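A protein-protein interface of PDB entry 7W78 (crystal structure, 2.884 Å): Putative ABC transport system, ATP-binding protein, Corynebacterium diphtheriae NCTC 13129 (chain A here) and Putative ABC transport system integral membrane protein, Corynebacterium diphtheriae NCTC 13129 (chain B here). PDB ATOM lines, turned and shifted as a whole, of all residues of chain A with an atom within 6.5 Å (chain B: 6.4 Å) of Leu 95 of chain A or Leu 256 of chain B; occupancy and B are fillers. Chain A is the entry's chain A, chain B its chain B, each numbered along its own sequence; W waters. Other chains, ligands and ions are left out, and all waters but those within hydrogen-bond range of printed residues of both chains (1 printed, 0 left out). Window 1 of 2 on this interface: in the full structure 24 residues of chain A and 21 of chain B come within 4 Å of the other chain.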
ATOM      1  N   ARG A  81      21.294 -15.183  -6.393  1.00  0.00           N
ATOM      2  CA  ARG A  81      20.037 -14.447  -6.506  1.00  0.00           C
ATOM      3  C   ARG A  81      20.190 -13.022  -5.990  1.00  0.00           C
ATOM      4  O   ARG A  81      19.775 -12.061  -6.649  1.00  0.00           O
ATOM      5  CB  ARG A  81      18.924 -15.174  -5.745  1.00  0.00           C
ATOM      6  CG  ARG A  81      18.682 -16.603  -6.204  1.00  0.00           C
ATOM      7  CD  ARG A  81      17.418 -17.201  -5.596  1.00  0.00           C
ATOM      8  NE  ARG A  81      17.459 -17.281  -4.141  1.00  0.00           N
ATOM      9  CZ  ARG A  81      17.915 -18.331  -3.466  1.00  0.00           C
ATOM     10  NH1 ARG A  81      18.378 -19.389  -4.118  1.00  0.00           N
ATOM     11  NH2 ARG A  81      17.912 -18.323  -2.141  1.00  0.00           N
ATOM     12  N   PRO A  92       2.110 -11.451  -6.874  1.00  0.00           N
ATOM     13  CA  PRO A  92       2.924 -10.291  -6.467  1.00  0.00           C
ATOM     14  C   PRO A  92       3.929 -10.593  -5.364  1.00  0.00           C
ATOM     15  O   PRO A  92       5.021 -10.011  -5.369  1.00  0.00           O
ATOM     16  CB  PRO A  92       1.874  -9.266  -6.016  1.00  0.00           C
ATOM     17  CG  PRO A  92       0.604  -9.697  -6.693  1.00  0.00           C
ATOM     18  CD  PRO A  92       0.669 -11.190  -6.720  1.00  0.00           C
ATOM     19  N   ASN A  93       3.599 -11.484  -4.428  1.00  0.00           N
ATOM     20  CA  ASN A  93       4.515 -11.890  -3.359  1.00  0.00           C
ATOM     21  C   ASN A  93       5.035 -10.683  -2.575  1.00  0.00           C
ATOM     22  O   ASN A  93       6.239 -10.505  -2.383  1.00  0.00           O
ATOM     23  CB  ASN A  93       5.684 -12.709  -3.915  1.00  0.00           C
ATOM     24  CG  ASN A  93       5.366 -14.189  -4.031  1.00  0.00           C
ATOM     25  OD1 ASN A  93       4.374 -14.671  -3.486  1.00  0.00           O
ATOM     26  ND2 ASN A  93       6.226 -14.920  -4.729  1.00  0.00           N
ATOM     27  N   LEU A  94       4.109  -9.843  -2.119  1.00  0.00           N
ATOM     28  CA  LEU A  94       4.457  -8.679  -1.318  1.00  0.00           C
ATOM     29  C   LEU A  94       4.438  -9.036   0.163  1.00  0.00           C
ATOM     30  O   LEU A  94       3.563  -9.774   0.624  1.00  0.00           O
ATOM     31  CB  LEU A  94       3.489  -7.527  -1.588  1.00  0.00           C
ATOM     32  CG  LEU A  94       3.383  -7.023  -3.028  1.00  0.00           C
ATOM     33  CD1 LEU A  94       2.347  -5.914  -3.123  1.00  0.00           C
ATOM     34  CD2 LEU A  94       4.730  -6.546  -3.532  1.00  0.00           C
ATOM     35  N   LEU A  95       5.409  -8.507   0.906  1.00  0.00           N
ATOM     36  CA  LEU A  95       5.498  -8.771   2.335  1.00  0.00           C
ATOM     37  C   LEU A  95       4.424  -7.982   3.077  1.00  0.00           C
ATOM     38  O   LEU A  95       4.271  -6.774   2.868  1.00  0.00           O
ATOM     39  CB  LEU A  95       6.891  -8.423   2.859  1.00  0.00           C
ATOM     40  CG  LEU A  95       8.051  -9.161   2.182  1.00  0.00           C
ATOM     41  CD1 LEU A  95       9.393  -8.666   2.695  1.00  0.00           C
ATOM     42  CD2 LEU A  95       7.930 -10.664   2.362  1.00  0.00           C
ATOM     43  N   GLY A  96       3.700  -8.670   3.965  1.00  0.00           N
ATOM     44  CA  GLY A  96       2.420  -8.170   4.444  1.00  0.00           C
ATOM     45  C   GLY A  96       2.475  -6.843   5.178  1.00  0.00           C
ATOM     46  O   GLY A  96       1.536  -6.046   5.089  1.00  0.00           O
ATOM     47  N   SER A  97       3.552  -6.584   5.915  1.00  0.00           N
ATOM     48  CA  SER A  97       3.596  -5.435   6.812  1.00  0.00           C
ATOM     49  C   SER A  97       4.314  -4.225   6.228  1.00  0.00           C
ATOM     50  O   SER A  97       4.352  -3.176   6.880  1.00  0.00           O
ATOM     51  CB  SER A  97       4.250  -5.826   8.139  1.00  0.00           C
ATOM     52  OG  SER A  97       5.471  -6.506   7.926  1.00  0.00           O
ATOM     53  N   LEU A  98       4.877  -4.331   5.034  1.00  0.00           N
ATOM     54  CA  LEU A  98       5.597  -3.205   4.461  1.00  0.00           C
ATOM     55  C   LEU A  98       4.667  -2.347   3.614  1.00  0.00           C
ATOM     56  O   LEU A  98       3.608  -2.789   3.162  1.00  0.00           O
ATOM     57  CB  LEU A  98       6.774  -3.695   3.619  1.00  0.00           C
ATOM     58  CG  LEU A  98       7.730  -4.648   4.337  1.00  0.00           C
ATOM     59  CD1 LEU A  98       8.814  -5.134   3.390  1.00  0.00           C
ATOM     60  CD2 LEU A  98       8.337  -3.981   5.561  1.00  0.00           C
ATOM     61  N   THR A  99       5.065  -1.096   3.420  1.00  0.00           N
ATOM     62  CA  THR A  99       4.372  -0.253   2.460  1.00  0.00           C
ATOM     63  C   THR A  99       4.983  -0.465   1.079  1.00  0.00           C
ATOM     64  O   THR A  99       6.072  -1.028   0.942  1.00  0.00           O
ATOM     65  CB  THR A  99       4.434   1.225   2.857  1.00  0.00           C
ATOM     66  OG1 THR A  99       5.746   1.744   2.609  1.00  0.00           O
ATOM     67  CG2 THR A  99       4.082   1.402   4.331  1.00  0.00           C
ATOM     68  N   GLN A 103       8.467  -2.116   0.187  1.00  0.00           N
ATOM     69  CA  GLN A 103       8.622  -3.342  -0.588  1.00  0.00           C
ATOM     70  C   GLN A 103       9.864  -3.290  -1.464  1.00  0.00           C
ATOM     71  O   GLN A 103      10.509  -4.320  -1.695  1.00  0.00           O
ATOM     72  CB  GLN A 103       7.385  -3.583  -1.454  1.00  0.00           C
ATOM     73  CG  GLN A 103       6.085  -3.738  -0.683  1.00  0.00           C
ATOM     74  CD  GLN A 103       5.959  -5.088  -0.001  1.00  0.00           C
ATOM     75  OE1 GLN A 103       6.865  -5.918  -0.061  1.00  0.00           O
ATOM     76  NE2 GLN A 103       4.824  -5.314   0.649  1.00  0.00           N
ATOM     77  N   ILE A 106      13.385  -2.821   1.122  1.00  0.00           N
ATOM     78  CA  ILE A 106      13.912  -3.954   1.877  1.00  0.00           C
ATOM     79  C   ILE A 106      14.921  -4.745   1.054  1.00  0.00           C
ATOM     80  O   ILE A 106      15.819  -5.382   1.615  1.00  0.00           O
ATOM     81  CB  ILE A 106      12.766  -4.850   2.387  1.00  0.00           C
ATOM     82  CG1 ILE A 106      13.306  -5.857   3.405  1.00  0.00           C
ATOM     83  CG2 ILE A 106      12.069  -5.563   1.238  1.00  0.00           C
ATOM     84  CD1 ILE A 106      12.246  -6.694   4.073  1.00  0.00           C
ATOM     85  N   THR A 107      14.817  -4.709  -0.278  1.00  0.00           N
ATOM     86  CA  THR A 107      15.817  -5.391  -1.095  1.00  0.00           C
ATOM     87  C   THR A 107      17.182  -4.727  -0.954  1.00  0.00           C
ATOM     88  O   THR A 107      18.210  -5.412  -0.933  1.00  0.00           O
ATOM     89  CB  THR A 107      15.377  -5.433  -2.558  1.00  0.00           C
ATOM     90  OG1 THR A 107      15.076  -4.110  -3.017  1.00  0.00           O
ATOM     91  CG2 THR A 107      14.154  -6.319  -2.717  1.00  0.00           C
ATOM     92  N   LEU A 110      18.471  -6.172   2.458  1.00  0.00           N
ATOM     93  CA  LEU A 110      19.030  -7.519   2.410  1.00  0.00           C
ATOM     94  C   LEU A 110      20.318  -7.566   1.598  1.00  0.00           C
ATOM     95  O   LEU A 110      21.171  -8.427   1.841  1.00  0.00           O
ATOM     96  CB  LEU A 110      17.995  -8.503   1.857  1.00  0.00           C
ATOM     97  CG  LEU A 110      17.605  -8.515   0.374  1.00  0.00           C
ATOM     98  CD1 LEU A 110      18.481  -9.468  -0.429  1.00  0.00           C
ATOM     99  CD2 LEU A 110      16.134  -8.872   0.224  1.00  0.00           C
ATOM    100  N   ARG A 136      -0.375   0.205   1.956  1.00  0.00           N
ATOM    101  CA  ARG A 136      -0.155  -1.165   2.381  1.00  0.00           C
ATOM    102  C   ARG A 136      -0.801  -2.102   1.367  1.00  0.00           C
ATOM    103  O   ARG A 136      -1.646  -1.696   0.566  1.00  0.00           O
ATOM    104  CB  ARG A 136      -0.710  -1.386   3.790  1.00  0.00           C
ATOM    105  CG  ARG A 136      -0.097  -0.447   4.835  1.00  0.00           C
ATOM    106  CD  ARG A 136      -0.194  -1.000   6.248  1.00  0.00           C
ATOM    107  NE  ARG A 136       0.229  -2.395   6.313  1.00  0.00           N
ATOM    108  CZ  ARG A 136      -0.017  -3.208   7.336  1.00  0.00           C
ATOM    109  NH1 ARG A 136      -0.682  -2.767   8.398  1.00  0.00           N
ATOM    110  NH2 ARG A 136       0.407  -4.465   7.300  1.00  0.00           N
ATOM    111  N   VAL A 137      -0.362  -3.365   1.384  1.00  0.00           N
ATOM    112  CA  VAL A 137      -0.811  -4.335   0.386  1.00  0.00           C
ATOM    113  C   VAL A 137      -2.329  -4.410   0.330  1.00  0.00           C
ATOM    114  O   VAL A 137      -2.914  -4.598  -0.744  1.00  0.00           O
ATOM    115  CB  VAL A 137      -0.194  -5.721   0.673  1.00  0.00           C
ATOM    116  CG1 VAL A 137      -0.634  -6.728  -0.381  1.00  0.00           C
ATOM    117  CG2 VAL A 137       1.321  -5.625   0.742  1.00  0.00           C
ATOM    118  N   ARG A 152      10.017  -3.687  -7.689  1.00  0.00           N
ATOM    119  CA  ARG A 152      10.981  -4.280  -6.769  1.00  0.00           C
ATOM    120  C   ARG A 152      12.087  -5.021  -7.508  1.00  0.00           C
ATOM    121  O   ARG A 152      13.227  -5.064  -7.033  1.00  0.00           O
ATOM    122  CB  ARG A 152      10.282  -5.226  -5.797  1.00  0.00           C
ATOM    123  CG  ARG A 152      11.237  -5.859  -4.805  1.00  0.00           C
ATOM    124  CD  ARG A 152      10.546  -6.906  -3.962  1.00  0.00           C
ATOM    125  NE  ARG A 152       9.690  -7.767  -4.769  1.00  0.00           N
ATOM    126  CZ  ARG A 152       8.771  -8.582  -4.263  1.00  0.00           C
ATOM    127  NH1 ARG A 152       8.594  -8.649  -2.951  1.00  0.00           N
ATOM    128  NH2 ARG A 152       8.032  -9.332  -5.066  1.00  0.00           N
ATOM    129  N   LEU B   3      12.447  -5.820   8.140  1.00  0.00           N
ATOM    130  CA  LEU B   3      11.085  -6.337   8.214  1.00  0.00           C
ATOM    131  C   LEU B   3      10.691  -6.646   9.651  1.00  0.00           C
ATOM    132  O   LEU B   3       9.570  -6.341  10.074  1.00  0.00           O
ATOM    133  CB  LEU B   3      10.952  -7.588   7.346  1.00  0.00           C
ATOM    134  CG  LEU B   3       9.595  -8.295   7.345  1.00  0.00           C
ATOM    135  CD1 LEU B   3       8.505  -7.363   6.846  1.00  0.00           C
ATOM    136  CD2 LEU B   3       9.645  -9.564   6.507  1.00  0.00           C
ATOM    137  N   ARG B 249       5.737 -16.925  10.087  1.00  0.00           N
ATOM    138  CA  ARG B 249       6.446 -16.079   9.139  1.00  0.00           C
ATOM    139  C   ARG B 249       7.124 -16.864   8.027  1.00  0.00           C
ATOM    140  O   ARG B 249       7.807 -16.250   7.199  1.00  0.00           O
ATOM    141  CB  ARG B 249       7.507 -15.235   9.852  1.00  0.00           C
ATOM    142  CG  ARG B 249       7.145 -14.790  11.247  1.00  0.00           C
ATOM    143  CD  ARG B 249       8.326 -14.090  11.902  1.00  0.00           C
ATOM    144  NE  ARG B 249       8.723 -12.881  11.186  1.00  0.00           N
ATOM    145  CZ  ARG B 249       9.943 -12.354  11.228  1.00  0.00           C
ATOM    146  NH1 ARG B 249      10.893 -12.936  11.946  1.00  0.00           N
ATOM    147  NH2 ARG B 249      10.213 -11.246  10.554  1.00  0.00           N
ATOM    148  N   ARG B 251       6.347 -17.914   5.311  1.00  0.00           N
ATOM    149  CA  ARG B 251       6.085 -17.495   3.951  1.00  0.00           C
ATOM    150  C   ARG B 251       6.810 -16.191   3.607  1.00  0.00           C
ATOM    151  O   ARG B 251       7.381 -16.066   2.520  1.00  0.00           O
ATOM    152  CB  ARG B 251       4.583 -17.391   3.771  1.00  0.00           C
ATOM    153  CG  ARG B 251       4.236 -16.869   2.476  1.00  0.00           C
ATOM    154  CD  ARG B 251       3.926 -15.402   2.637  1.00  0.00           C
ATOM    155  NE  ARG B 251       3.586 -14.860   1.336  1.00  0.00           N
ATOM    156  CZ  ARG B 251       3.805 -13.610   0.980  1.00  0.00           C
ATOM    157  NH1 ARG B 251       4.369 -12.785   1.805  1.00  0.00           N
ATOM    158  NH2 ARG B 251       3.479 -13.208  -0.199  1.00  0.00           N
ATOM    159  N   ASP B 252       6.797 -15.207   4.511  1.00  0.00           N
ATOM    160  CA  ASP B 252       7.550 -13.988   4.213  1.00  0.00           C
ATOM    161  C   ASP B 252       9.053 -14.231   4.305  1.00  0.00           C
ATOM    162  O   ASP B 252       9.825 -13.604   3.569  1.00  0.00           O
ATOM    163  CB  ASP B 252       7.111 -12.837   5.125  1.00  0.00           C
ATOM    164  CG  ASP B 252       5.828 -12.191   4.643  1.00  0.00           C
ATOM    165  OD1 ASP B 252       5.208 -11.367   5.354  1.00  0.00           O
ATOM    166  OD2 ASP B 252       5.434 -12.530   3.518  1.00  0.00           O
ATOM    167  N   ILE B 253       9.474 -15.158   5.163  1.00  0.00           N
ATOM    168  CA  ILE B 253      10.873 -15.570   5.141  1.00  0.00           C
ATOM    169  C   ILE B 253      11.201 -16.253   3.822  1.00  0.00           C
ATOM    170  O   ILE B 253      12.236 -15.974   3.207  1.00  0.00           O
ATOM    171  CB  ILE B 253      11.197 -16.470   6.347  1.00  0.00           C
ATOM    172  CG1 ILE B 253      10.971 -15.698   7.647  1.00  0.00           C
ATOM    173  CG2 ILE B 253      12.642 -16.958   6.266  1.00  0.00           C
ATOM    174  CD1 ILE B 253      11.136 -16.521   8.893  1.00  0.00           C
ATOM    175  N   ALA B 254      10.308 -17.129   3.347  1.00  0.00           N
ATOM    176  CA  ALA B 254      10.508 -17.770   2.049  1.00  0.00           C
ATOM    177  C   ALA B 254      10.670 -16.738   0.937  1.00  0.00           C
ATOM    178  O   ALA B 254      11.519 -16.899   0.053  1.00  0.00           O
ATOM    179  CB  ALA B 254       9.343 -18.707   1.735  1.00  0.00           C
ATOM    180  N   VAL B 255       9.868 -15.672   0.966  1.00  0.00           N
ATOM    181  CA  VAL B 255       9.947 -14.667  -0.090  1.00  0.00           C
ATOM    182  C   VAL B 255      11.269 -13.911  -0.015  1.00  0.00           C
ATOM    183  O   VAL B 255      11.903 -13.642  -1.044  1.00  0.00           O
ATOM    184  CB  VAL B 255       8.734 -13.721  -0.019  1.00  0.00           C
ATOM    185  CG1 VAL B 255       9.015 -12.427  -0.764  1.00  0.00           C
ATOM    186  CG2 VAL B 255       7.504 -14.405  -0.594  1.00  0.00           C
ATOM    187  N   LEU B 256      11.714 -13.564   1.197  1.00  0.00           N
ATOM    188  CA  LEU B 256      13.012 -12.910   1.346  1.00  0.00           C
ATOM    189  C   LEU B 256      14.145 -13.823   0.898  1.00  0.00           C
ATOM    190  O   LEU B 256      15.099 -13.373   0.253  1.00  0.00           O
ATOM    191  CB  LEU B 256      13.223 -12.475   2.795  1.00  0.00           C
ATOM    192  CG  LEU B 256      12.468 -11.233   3.269  1.00  0.00           C
ATOM    193  CD1 LEU B 256      12.534 -11.121   4.782  1.00  0.00           C
ATOM    194  CD2 LEU B 256      13.042  -9.991   2.614  1.00  0.00           C
ATOM    195  N   ALA B 257      14.061 -15.110   1.241  1.00  0.00           N
ATOM    196  CA  ALA B 257      15.066 -16.068   0.788  1.00  0.00           C
ATOM    197  C   ALA B 257      15.129 -16.109  -0.733  1.00  0.00           C
ATOM    198  O   ALA B 257      16.216 -16.094  -1.320  1.00  0.00           O
ATOM    199  CB  ALA B 257      14.761 -17.456   1.351  1.00  0.00           C
ATOM    200  N   ALA B 258      13.963 -16.151  -1.387  1.00  0.00           N
ATOM    201  CA  ALA B 258      13.935 -16.211  -2.847  1.00  0.00           C
ATOM    202  C   ALA B 258      14.634 -15.007  -3.464  1.00  0.00           C
ATOM    203  O   ALA B 258      15.332 -15.137  -4.476  1.00  0.00           O
ATOM    204  CB  ALA B 258      12.492 -16.311  -3.346  1.00  0.00           C
ATOM    205  N   LEU B 259      14.475 -13.827  -2.864  1.00  0.00           N
ATOM    206  CA  LEU B 259      15.091 -12.630  -3.420  1.00  0.00           C
ATOM    207  C   LEU B 259      16.595 -12.571  -3.178  1.00  0.00           C
ATOM    208  O   LEU B 259      17.293 -11.840  -3.889  1.00  0.00           O
ATOM    209  CB  LEU B 259      14.426 -11.380  -2.847  1.00  0.00           C
ATOM    210  CG  LEU B 259      12.939 -11.237  -3.170  1.00  0.00           C
ATOM    211  CD1 LEU B 259      12.400  -9.926  -2.643  1.00  0.00           C
ATOM    212  CD2 LEU B 259      12.704 -11.364  -4.659  1.00  0.00           C
ATOM    213  N   GLY B 260      17.105 -13.314  -2.198  1.00  0.00           N
ATOM    214  CA  GLY B 260      18.537 -13.387  -1.991  1.00  0.00           C
ATOM    215  C   GLY B 260      18.996 -13.210  -0.559  1.00  0.00           C
ATOM    216  O   GLY B 260      20.201 -13.123  -0.306  1.00  0.00           O
ATOM    217  N   ALA B 261      18.060 -13.158   0.387  1.00  0.00           N
ATOM    218  CA  ALA B 261      18.432 -12.972   1.783  1.00  0.00           C
ATOM    219  C   ALA B 261      19.258 -14.152   2.277  1.00  0.00           C
ATOM    220  O   ALA B 261      18.852 -15.310   2.147  1.00  0.00           O
ATOM    221  CB  ALA B 261      17.184 -12.800   2.650  1.00  0.00           C
ATOM    222  N   SER B 262      20.434 -13.854   2.823  1.00  0.00           N
ATOM    223  CA  SER B 262      21.245 -14.888   3.442  1.00  0.00           C
ATOM    224  C   SER B 262      20.554 -15.402   4.700  1.00  0.00           C
ATOM    225  O   SER B 262      19.721 -14.720   5.303  1.00  0.00           O
ATOM    226  CB  SER B 262      22.633 -14.351   3.792  1.00  0.00           C
ATOM    227  OG  SER B 262      22.599 -13.612   5.000  1.00  0.00           O
ATOM    228  N   TYR B 265      21.159 -13.075   7.623  1.00  0.00           N
ATOM    229  CA  TYR B 265      20.212 -11.964   7.586  1.00  0.00           C
ATOM    230  C   TYR B 265      18.861 -12.376   8.155  1.00  0.00           C
ATOM    231  O   TYR B 265      18.269 -11.665   8.975  1.00  0.00           O
ATOM    232  CB  TYR B 265      20.052 -11.465   6.150  1.00  0.00           C
ATOM    233  CG  TYR B 265      19.107 -10.296   6.034  1.00  0.00           C
ATOM    234  CD1 TYR B 265      17.774 -10.482   5.691  1.00  0.00           C
ATOM    235  CD2 TYR B 265      19.546  -9.005   6.283  1.00  0.00           C
ATOM    236  CE1 TYR B 265      16.908  -9.410   5.592  1.00  0.00           C
ATOM    237  CE2 TYR B 265      18.692  -7.931   6.187  1.00  0.00           C
ATOM    238  CZ  TYR B 265      17.374  -8.136   5.842  1.00  0.00           C
ATOM    239  OH  TYR B 265      16.522  -7.061   5.750  1.00  0.00           O
ATOM    240  N   LEU B 266      18.362 -13.538   7.732  1.00  0.00           N
ATOM    241  CA  LEU B 266      17.041 -13.978   8.161  1.00  0.00           C
ATOM    242  C   LEU B 266      17.020 -14.327   9.642  1.00  0.00           C
ATOM    243  O   LEU B 266      16.061 -13.995  10.347  1.00  0.00           O
ATOM    244  CB  LEU B 266      16.598 -15.167   7.315  1.00  0.00           C
ATOM    245  CG  LEU B 266      16.407 -14.748   5.860  1.00  0.00           C
ATOM    246  CD1 LEU B 266      16.107 -15.943   4.975  1.00  0.00           C
ATOM    247  CD2 LEU B 266      15.301 -13.707   5.778  1.00  0.00           C
ATOM    248  N   ASP B 269      17.235 -11.040  11.651  1.00  0.00           N
ATOM    249  CA  ASP B 269      15.904 -10.440  11.628  1.00  0.00           C
ATOM    250  C   ASP B 269      14.972 -11.151  12.599  1.00  0.00           C
ATOM    251  O   ASP B 269      14.259 -10.510  13.378  1.00  0.00           O
ATOM    252  CB  ASP B 269      15.329 -10.487  10.212  1.00  0.00           C
ATOM    253  CG  ASP B 269      13.971  -9.802  10.106  1.00  0.00           C
ATOM    254  OD1 ASP B 269      12.965 -10.382  10.569  1.00  0.00           O
ATOM    255  OD2 ASP B 269      13.908  -8.687   9.546  1.00  0.00           O
HETATM  256  O   HOH W   1       2.596 -11.711   4.306  1.00  0.00           O
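Water W1 lies within hydrogen-bond range of the side-chain carboxylate of Asp 252 of chain B (2.8 Å), the guanidinium group of Arg 251 of chain B (3.2 Å) and the backbone NH of Gly 96 of chain A (3.3 Å).
The backbone NH (N) of Gly 96 of chain A lies within hydrogen-bond range of the side-chain carboxylate (OD1) of Asp 252 of chain B (3.4 Å). The backbone carbonyl oxygen (O) of Ala 258 of chain B is in hydrogen-bond range of the guanidinium group (NE) of Arg 81 of chain A. The backbone carbonyl oxygen (O) of Ala 257 of chain B sits at hydrogen-bond distance from the guanidinium group (NH2) of Arg 81 of chain A, 2.9 Å away. The guanidinium group (NH1) of Arg 251 of chain B lies within hydrogen-bond range of the backbone carbonyl oxygen (O) of Leu 94 of chain A, at 3.3 Å.
Of the printed residues of chain B, Arg 81 of chain A touches Ala 257 (2.9 Å), Ala 258 (3.0 Å) and Leu 259 (3.7 Å). Of the printed residues of chain B, Leu 94 of chain A touches Arg 251 (3.3 Å). Of chain B, only Leu 3, Asp 252, Val 255 and Leu 256 come within 4 Å of Leu 95 of chain A. Of the printed residues of chain B, Gly 96 of chain A touches Asp 252. Val 137 of chain A touches none of the printed residues of chain B. Of the printed residues of chain A, Leu 3 of chain B touches Leu 95 (3.9 Å), Ser 97 (3.3 Å), Leu 98 (3.6 Å) and Ile 106 (3.6 Å). Ala 254 of chain B touches none of the printed residues of chain A. Of chain A, only Leu 95 (3.9 Å) and Ile 106 (3.7 Å) come within 4 Å of Leu 256 of chain B. Printed residues of chain A within 4 Å of Ala 257 of chain B: Arg 81. The nearest residue of chain B that does not touch Leu 95 of chain A is Arg 251 of chain B (4.2 Å). The nearest printed residue of chain A that does not touch Leu 3 of chain B is Gly 96 of chain A (5.8 Å).
Along chain A the printed residues that touch a printed residue of chain B span positions 81 to 152. Hydrophobic or aromatic side chains of chain B within 4 Å of the printed part of chain A: Leu 3, Val 255, Leu 256, Leu 259 and Tyr 265. Among the printed residues, 19 pairs touch across the chains.
N of Ala 261 of chain B lies within hydrogen-bond range of O of Leu 256 of chain B (3.0 Å). The backbone carbonyl oxygen (O) of Pro 92 of chain A sits at hydrogen-bond distance from the guanidinium group (NH2) of Arg 152 of chain A (3.1 Å). The side-chain carboxylate of Asp 252 of chain B lies within salt-bridge range of the guanidinium group of Arg 251 of chain B, 3.7 Å away. The backbone NH (N) of Tyr 265 of chain B sits at hydrogen-bond distance from the side-chain hydroxyl (OG) of Ser 262 of chain B (3.0 Å). O of Gly 96 of chain A lies within hydrogen-bond range of NH2 of Arg 136 of chain A, 2.9 Å away. The side-chain amide nitrogen (NE2) of Gln 103 of chain A is in hydrogen-bond range of the backbone carbonyl oxygen (O) of Leu 95 of chain A, at 2.7 Å.
Among the printed residues, merely in contact across the chains: Leu 95 of chain A with Asp 252 of chain B (3.3 Å), Ser 97 of chain A with Leu 3 of chain B (3.3 Å), Asn 93 of chain A with Arg 251 of chain B (3.6 Å), Leu 98 of chain A with Leu 3 of chain B (3.6 Å), Ile 106 of chain A with Leu 3 of chain B (3.6 Å), Ile 106 of chain A with Leu 256 of chain B (3.7 Å), Arg 81 of chain A with Leu 259 of chain B (3.7 Å), Asn 93 of chain A with Val 255 of chain B (3.7 Å), Leu 95 of chain A with Val 255 of chain B (3.7 Å), Leu 110 of chain A with Gly 260 of chain B (3.8 Å), Arg 152 of chain A with Leu 259 of chain B (3.8 Å), Leu 110 of chain A with Ala 261 of chain B (3.8 Å), Leu 110 of chain A with Tyr 265 of chain B (3.8 Å), Leu 95 of chain A with Leu 256 of chain B (3.9 Å) and Leu 95 of chain A with Leu 3 of chain B (3.9 Å).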
